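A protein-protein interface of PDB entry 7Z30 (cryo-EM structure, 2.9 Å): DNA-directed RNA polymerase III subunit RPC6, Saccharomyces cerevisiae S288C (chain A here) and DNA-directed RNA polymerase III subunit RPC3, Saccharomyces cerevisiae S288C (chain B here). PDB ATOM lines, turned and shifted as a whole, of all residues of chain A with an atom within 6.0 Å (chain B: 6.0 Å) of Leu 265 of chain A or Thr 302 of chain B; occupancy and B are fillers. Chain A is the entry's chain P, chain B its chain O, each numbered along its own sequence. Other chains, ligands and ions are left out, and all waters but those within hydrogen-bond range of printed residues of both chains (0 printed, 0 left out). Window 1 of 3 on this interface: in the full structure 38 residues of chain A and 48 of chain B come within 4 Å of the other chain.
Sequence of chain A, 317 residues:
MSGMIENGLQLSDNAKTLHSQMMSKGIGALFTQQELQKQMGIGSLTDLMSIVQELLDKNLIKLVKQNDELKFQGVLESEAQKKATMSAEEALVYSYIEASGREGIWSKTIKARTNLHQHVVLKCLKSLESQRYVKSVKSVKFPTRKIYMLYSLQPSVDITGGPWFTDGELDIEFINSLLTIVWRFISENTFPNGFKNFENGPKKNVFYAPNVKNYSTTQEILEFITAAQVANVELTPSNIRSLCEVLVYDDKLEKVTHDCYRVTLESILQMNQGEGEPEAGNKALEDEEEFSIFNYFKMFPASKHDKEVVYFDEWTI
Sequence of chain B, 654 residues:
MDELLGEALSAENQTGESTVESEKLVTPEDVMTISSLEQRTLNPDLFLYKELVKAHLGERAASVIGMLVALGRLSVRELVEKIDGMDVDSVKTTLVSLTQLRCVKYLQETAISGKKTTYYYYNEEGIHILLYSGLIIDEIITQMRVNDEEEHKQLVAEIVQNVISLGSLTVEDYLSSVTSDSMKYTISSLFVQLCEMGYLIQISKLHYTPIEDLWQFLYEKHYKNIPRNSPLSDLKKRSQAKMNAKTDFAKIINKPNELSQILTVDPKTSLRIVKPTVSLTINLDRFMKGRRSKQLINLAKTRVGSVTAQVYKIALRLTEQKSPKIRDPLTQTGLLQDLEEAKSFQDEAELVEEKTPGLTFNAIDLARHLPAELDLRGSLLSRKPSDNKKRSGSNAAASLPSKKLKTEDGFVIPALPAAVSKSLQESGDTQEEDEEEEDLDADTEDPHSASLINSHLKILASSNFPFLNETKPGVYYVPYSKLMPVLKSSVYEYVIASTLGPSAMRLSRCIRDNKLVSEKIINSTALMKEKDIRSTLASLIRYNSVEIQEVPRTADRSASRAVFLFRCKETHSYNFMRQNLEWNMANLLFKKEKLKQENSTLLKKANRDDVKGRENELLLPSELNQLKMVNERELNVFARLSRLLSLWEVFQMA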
ATOM      1  N   ASP A 251      -9.403  30.538  -4.876  1.00  0.00           N
ATOM      2  CA  ASP A 251      -9.214  29.432  -3.936  1.00  0.00           C
ATOM      3  C   ASP A 251      -8.360  28.330  -4.560  1.00  0.00           C
ATOM      4  O   ASP A 251      -8.789  27.185  -4.715  1.00  0.00           O
ATOM      5  CB  ASP A 251     -10.557  28.879  -3.449  1.00  0.00           C
ATOM      6  CG  ASP A 251     -10.513  28.432  -2.002  1.00  0.00           C
ATOM      7  OD1 ASP A 251      -9.404  28.175  -1.490  1.00  0.00           O
ATOM      8  OD2 ASP A 251     -11.589  28.333  -1.376  1.00  0.00           O
ATOM      9  N   VAL A 263      -2.928  23.451  -0.682  1.00  0.00           N
ATOM     10  CA  VAL A 263      -4.327  23.267  -1.047  1.00  0.00           C
ATOM     11  C   VAL A 263      -5.008  22.459   0.049  1.00  0.00           C
ATOM     12  O   VAL A 263      -4.406  21.551   0.633  1.00  0.00           O
ATOM     13  CB  VAL A 263      -4.484  22.583  -2.422  1.00  0.00           C
ATOM     14  CG1 VAL A 263      -3.750  23.367  -3.488  1.00  0.00           C
ATOM     15  CG2 VAL A 263      -3.969  21.161  -2.384  1.00  0.00           C
ATOM     16  N   THR A 264      -6.257  22.812   0.349  1.00  0.00           N
ATOM     17  CA  THR A 264      -7.010  22.164   1.417  1.00  0.00           C
ATOM     18  C   THR A 264      -8.257  21.453   0.915  1.00  0.00           C
ATOM     19  O   THR A 264      -8.479  20.286   1.258  1.00  0.00           O
ATOM     20  CB  THR A 264      -7.392  23.192   2.496  1.00  0.00           C
ATOM     21  OG1 THR A 264      -8.627  23.828   2.142  1.00  0.00           O
ATOM     22  CG2 THR A 264      -6.307  24.246   2.649  1.00  0.00           C
ATOM     23  N   LEU A 265      -9.079  22.120   0.105  1.00  0.00           N
ATOM     24  CA  LEU A 265     -10.344  21.565  -0.363  1.00  0.00           C
ATOM     25  C   LEU A 265     -10.434  21.553  -1.886  1.00  0.00           C
ATOM     26  O   LEU A 265     -11.530  21.517  -2.453  1.00  0.00           O
ATOM     27  CB  LEU A 265     -11.515  22.334   0.247  1.00  0.00           C
ATOM     28  CG  LEU A 265     -11.949  23.682  -0.335  1.00  0.00           C
ATOM     29  CD1 LEU A 265     -13.415  23.938  -0.017  1.00  0.00           C
ATOM     30  CD2 LEU A 265     -11.078  24.812   0.183  1.00  0.00           C
ATOM     31  N   GLU A 266      -9.282  21.564  -2.557  1.00  0.00           N
ATOM     32  CA  GLU A 266      -9.275  21.566  -4.015  1.00  0.00           C
ATOM     33  C   GLU A 266      -9.899  20.296  -4.575  1.00  0.00           C
ATOM     34  O   GLU A 266     -10.680  20.355  -5.531  1.00  0.00           O
ATOM     35  CB  GLU A 266      -7.845  21.734  -4.526  1.00  0.00           C
ATOM     36  CG  GLU A 266      -7.364  23.180  -4.606  1.00  0.00           C
ATOM     37  CD  GLU A 266      -7.964  23.960  -5.767  1.00  0.00           C
ATOM     38  OE1 GLU A 266      -9.134  23.722  -6.134  1.00  0.00           O
ATOM     39  OE2 GLU A 266      -7.248  24.817  -6.322  1.00  0.00           O
ATOM     40  N   SER A 267      -9.569  19.139  -3.996  1.00  0.00           N
ATOM     41  CA  SER A 267     -10.144  17.884  -4.471  1.00  0.00           C
ATOM     42  C   SER A 267     -11.649  17.842  -4.237  1.00  0.00           C
ATOM     43  O   SER A 267     -12.405  17.375  -5.097  1.00  0.00           O
ATOM     44  CB  SER A 267      -9.465  16.701  -3.787  1.00  0.00           C
ATOM     45  OG  SER A 267     -10.046  15.475  -4.195  1.00  0.00           O
ATOM     46  N   ILE A 268     -12.102  18.319  -3.075  1.00  0.00           N
ATOM     47  CA  ILE A 268     -13.534  18.353  -2.790  1.00  0.00           C
ATOM     48  C   ILE A 268     -14.248  19.260  -3.784  1.00  0.00           C
ATOM     49  O   ILE A 268     -15.354  18.954  -4.246  1.00  0.00           O
ATOM     50  CB  ILE A 268     -13.778  18.793  -1.335  1.00  0.00           C
ATOM     51  CG1 ILE A 268     -12.923  17.959  -0.378  1.00  0.00           C
ATOM     52  CG2 ILE A 268     -15.253  18.678  -0.979  1.00  0.00           C
ATOM     53  CD1 ILE A 268     -12.497  18.700   0.870  1.00  0.00           C
ATOM     54  N   LEU A 269     -13.628  20.392  -4.124  1.00  0.00           N
ATOM     55  CA  LEU A 269     -14.193  21.282  -5.132  1.00  0.00           C
ATOM     56  C   LEU A 269     -14.258  20.605  -6.496  1.00  0.00           C
ATOM     57  O   LEU A 269     -15.263  20.714  -7.210  1.00  0.00           O
ATOM     58  CB  LEU A 269     -13.368  22.568  -5.203  1.00  0.00           C
ATOM     59  CG  LEU A 269     -13.902  23.713  -6.063  1.00  0.00           C
ATOM     60  CD1 LEU A 269     -13.774  25.040  -5.335  1.00  0.00           C
ATOM     61  CD2 LEU A 269     -13.165  23.761  -7.392  1.00  0.00           C
ATOM     62  N   GLN A 270     -13.192  19.899  -6.877  1.00  0.00           N
ATOM     63  CA  GLN A 270     -13.127  19.312  -8.213  1.00  0.00           C
ATOM     64  C   GLN A 270     -14.099  18.149  -8.368  1.00  0.00           C
ATOM     65  O   GLN A 270     -14.719  17.990  -9.427  1.00  0.00           O
ATOM     66  CB  GLN A 270     -11.696  18.872  -8.518  1.00  0.00           C
ATOM     67  CG  GLN A 270     -10.723  20.027  -8.693  1.00  0.00           C
ATOM     68  CD  GLN A 270     -10.935  20.784  -9.993  1.00  0.00           C
ATOM     69  OE1 GLN A 270     -11.925  21.498 -10.160  1.00  0.00           O
ATOM     70  NE2 GLN A 270      -9.997  20.635 -10.921  1.00  0.00           N
ATOM     71  N   SER A 292     -22.640  23.532   5.425  1.00  0.00           N
ATOM     72  CA  SER A 292     -21.313  23.316   4.848  1.00  0.00           C
ATOM     73  C   SER A 292     -21.077  24.295   3.694  1.00  0.00           C
ATOM     74  O   SER A 292     -20.949  23.921   2.524  1.00  0.00           O
ATOM     75  CB  SER A 292     -21.139  21.864   4.384  1.00  0.00           C
ATOM     76  OG  SER A 292     -21.615  21.702   3.062  1.00  0.00           O
ATOM     77  N   ILE A 293     -21.043  25.577   4.070  1.00  0.00           N
ATOM     78  CA  ILE A 293     -21.071  26.648   3.081  1.00  0.00           C
ATOM     79  C   ILE A 293     -19.949  26.485   2.069  1.00  0.00           C
ATOM     80  O   ILE A 293     -20.210  26.471   0.862  1.00  0.00           O
ATOM     81  CB  ILE A 293     -21.003  28.031   3.764  1.00  0.00           C
ATOM     82  CG1 ILE A 293     -21.922  28.119   4.988  1.00  0.00           C
ATOM     83  CG2 ILE A 293     -21.336  29.125   2.767  1.00  0.00           C
ATOM     84  CD1 ILE A 293     -21.258  28.827   6.150  1.00  0.00           C
ATOM     85  N   PHE A 294     -18.709  26.260   2.532  1.00  0.00           N
ATOM     86  CA  PHE A 294     -17.516  26.348   1.688  1.00  0.00           C
ATOM     87  C   PHE A 294     -17.477  25.297   0.589  1.00  0.00           C
ATOM     88  O   PHE A 294     -16.466  25.206  -0.115  1.00  0.00           O
ATOM     89  CB  PHE A 294     -16.236  26.284   2.536  1.00  0.00           C
ATOM     90  CG  PHE A 294     -16.094  27.432   3.499  1.00  0.00           C
ATOM     91  CD1 PHE A 294     -16.694  27.380   4.745  1.00  0.00           C
ATOM     92  CD2 PHE A 294     -15.375  28.568   3.152  1.00  0.00           C
ATOM     93  CE1 PHE A 294     -16.580  28.433   5.630  1.00  0.00           C
ATOM     94  CE2 PHE A 294     -15.259  29.628   4.037  1.00  0.00           C
ATOM     95  CZ  PHE A 294     -15.861  29.560   5.276  1.00  0.00           C
ATOM     96  N   ASN A 295     -18.536  24.506   0.429  1.00  0.00           N
ATOM     97  CA  ASN A 295     -18.724  23.670  -0.754  1.00  0.00           C
ATOM     98  C   ASN A 295     -20.215  23.514  -1.019  1.00  0.00           C
ATOM     99  O   ASN A 295     -20.926  22.885  -0.229  1.00  0.00           O
ATOM    100  CB  ASN A 295     -18.036  22.306  -0.585  1.00  0.00           C
ATOM    101  CG  ASN A 295     -18.606  21.480   0.562  1.00  0.00           C
ATOM    102  OD1 ASN A 295     -19.082  22.015   1.567  1.00  0.00           O
ATOM    103  ND2 ASN A 295     -18.558  20.164   0.410  1.00  0.00           N
ATOM    104  N   ILE B 297     -16.413  23.406  13.012  1.00  0.00           N
ATOM    105  CA  ILE B 297     -16.219  21.990  12.709  1.00  0.00           C
ATOM    106  C   ILE B 297     -16.623  21.685  11.274  1.00  0.00           C
ATOM    107  O   ILE B 297     -15.939  20.936  10.568  1.00  0.00           O
ATOM    108  CB  ILE B 297     -16.991  21.109  13.710  1.00  0.00           C
ATOM    109  CG1 ILE B 297     -16.449  21.274  15.133  1.00  0.00           C
ATOM    110  CG2 ILE B 297     -16.960  19.653  13.278  1.00  0.00           C
ATOM    111  CD1 ILE B 297     -14.963  21.546  15.211  1.00  0.00           C
ATOM    112  N   ASN B 298     -17.747  22.243  10.822  1.00  0.00           N
ATOM    113  CA  ASN B 298     -18.141  22.038   9.432  1.00  0.00           C
ATOM    114  C   ASN B 298     -17.143  22.687   8.479  1.00  0.00           C
ATOM    115  O   ASN B 298     -16.863  22.147   7.402  1.00  0.00           O
ATOM    116  CB  ASN B 298     -19.548  22.572   9.182  1.00  0.00           C
ATOM    117  CG  ASN B 298     -20.361  21.651   8.302  1.00  0.00           C
ATOM    118  OD1 ASN B 298     -20.008  21.422   7.149  1.00  0.00           O
ATOM    119  ND2 ASN B 298     -21.459  21.130   8.830  1.00  0.00           N
ATOM    120  N   LEU B 299     -16.605  23.848   8.858  1.00  0.00           N
ATOM    121  CA  LEU B 299     -15.535  24.472   8.087  1.00  0.00           C
ATOM    122  C   LEU B 299     -14.337  23.538   7.961  1.00  0.00           C
ATOM    123  O   LEU B 299     -13.779  23.364   6.872  1.00  0.00           O
ATOM    124  CB  LEU B 299     -15.135  25.793   8.751  1.00  0.00           C
ATOM    125  CG  LEU B 299     -13.909  26.578   8.277  1.00  0.00           C
ATOM    126  CD1 LEU B 299     -14.172  28.067   8.400  1.00  0.00           C
ATOM    127  CD2 LEU B 299     -12.677  26.200   9.085  1.00  0.00           C
ATOM    128  N   ALA B 300     -13.931  22.926   9.076  1.00  0.00           N
ATOM    129  CA  ALA B 300     -12.806  21.996   9.053  1.00  0.00           C
ATOM    130  C   ALA B 300     -13.107  20.785   8.179  1.00  0.00           C
ATOM    131  O   ALA B 300     -12.239  20.318   7.433  1.00  0.00           O
ATOM    132  CB  ALA B 300     -12.458  21.561  10.476  1.00  0.00           C
ATOM    133  N   LYS B 301     -14.331  20.260   8.267  1.00  0.00           N
ATOM    134  CA  LYS B 301     -14.720  19.137   7.418  1.00  0.00           C
ATOM    135  C   LYS B 301     -14.647  19.516   5.946  1.00  0.00           C
ATOM    136  O   LYS B 301     -14.225  18.710   5.106  1.00  0.00           O
ATOM    137  CB  LYS B 301     -16.129  18.664   7.776  1.00  0.00           C
ATOM    138  CG  LYS B 301     -16.241  17.163   7.999  1.00  0.00           C
ATOM    139  CD  LYS B 301     -17.637  16.767   8.454  1.00  0.00           C
ATOM    140  CE  LYS B 301     -17.939  17.293   9.848  1.00  0.00           C
ATOM    141  NZ  LYS B 301     -19.207  16.735  10.394  1.00  0.00           N
ATOM    142  N   THR B 302     -15.056  20.739   5.612  1.00  0.00           N
ATOM    143  CA  THR B 302     -14.935  21.212   4.240  1.00  0.00           C
ATOM    144  C   THR B 302     -13.487  21.498   3.866  1.00  0.00           C
ATOM    145  O   THR B 302     -13.142  21.484   2.681  1.00  0.00           O
ATOM    146  CB  THR B 302     -15.784  22.471   4.041  1.00  0.00           C
ATOM    147  OG1 THR B 302     -17.058  22.293   4.674  1.00  0.00           O
ATOM    148  CG2 THR B 302     -16.006  22.734   2.563  1.00  0.00           C
ATOM    149  N   ARG B 303     -12.624  21.724   4.858  1.00  0.00           N
ATOM    150  CA  ARG B 303     -11.266  22.186   4.591  1.00  0.00           C
ATOM    151  C   ARG B 303     -10.258  21.043   4.645  1.00  0.00           C
ATOM    152  O   ARG B 303      -9.326  20.990   3.836  1.00  0.00           O
ATOM    153  CB  ARG B 303     -10.890  23.278   5.595  1.00  0.00           C
ATOM    154  CG  ARG B 303      -9.482  23.825   5.466  1.00  0.00           C
ATOM    155  CD  ARG B 303      -8.954  24.240   6.834  1.00  0.00           C
ATOM    156  NE  ARG B 303      -7.562  24.669   6.794  1.00  0.00           N
ATOM    157  CZ  ARG B 303      -7.092  25.736   7.427  1.00  0.00           C
ATOM    158  NH1 ARG B 303      -7.879  26.505   8.160  1.00  0.00           N
ATOM    159  NH2 ARG B 303      -5.801  26.036   7.322  1.00  0.00           N
ATOM    160  N   VAL B 304     -10.429  20.120   5.588  1.00  0.00           N
ATOM    161  CA  VAL B 304      -9.447  19.077   5.848  1.00  0.00           C
ATOM    162  C   VAL B 304     -10.152  17.725   5.845  1.00  0.00           C
ATOM    163  O   VAL B 304     -11.301  17.596   6.274  1.00  0.00           O
ATOM    164  CB  VAL B 304      -8.703  19.328   7.181  1.00  0.00           C
ATOM    165  CG1 VAL B 304      -8.216  18.036   7.804  1.00  0.00           C
ATOM    166  CG2 VAL B 304      -7.548  20.295   6.969  1.00  0.00           C
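Of the 8 printed residues of chain B, 4 touch a printed residue of chain A.
Hydrophobic or aromatic side chains of chain B that line the printed part of chain A: Leu 299.
Hydrophobic or aromatic side chains of chain A within 4 Å of the printed part of chain B: Leu 265, Ile 268 and Phe 294.
Among the printed residues, 8 pairs touch across the chains.
Among the printed residues, no Asp or Glu carboxylate lies within 4 Å of a Lys or Arg side-chain nitrogen of the other chain.
O of Arg 303 of chain B lies close to OG1 of Thr 264 of chain A (3.4 Å).
Leu 265 of chain A touches just these residues of chain B: Thr 302 (3.0 Å) and Arg 303 (3.9 Å).
Of the printed residues of chain B, Ser 292 of chain A touches Asn 298 (3.0 Å).
Of the printed residues of chain B, Phe 294 of chain A touches Leu 299 and Thr 302.
Printed residues of chain B within 4 Å of Asn 295 of chain A: Thr 302 (3.3 Å).
Printed residues of chain A within 4 Å of Asn 298 of chain B: Ser 292 (3.0 Å).
Val 304 of chain B touches none of the printed residues of chain A.
The nearest residue of chain A that does not touch Thr 302 of chain B is Ser 292 of chain A (4.1 Å).
The backbone carbonyl oxygen (O) of Asn 298 of chain B sits at hydrogen-bond distance from the side-chain hydroxyl (OG1) of Thr 302 of chain B (2.7 Å).
O of Ser 292 of chain A lies close to OD1 of Asn 295 of chain A, at 2.8 Å.
Among the printed residues, merely in contact across the chains: Ser 292 of chain A with Asn 298 of chain B, Leu 265 of chain A with Thr 302 of chain B, Asn 295 of chain A with Thr 302 of chain B, Ile 268 of chain A with Thr 302 of chain B, Phe 294 of chain A with Thr 302 of chain B, Phe 294 of chain A with Leu 299 of chain B and Leu 265 of chain A with Arg 303 of chain B.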
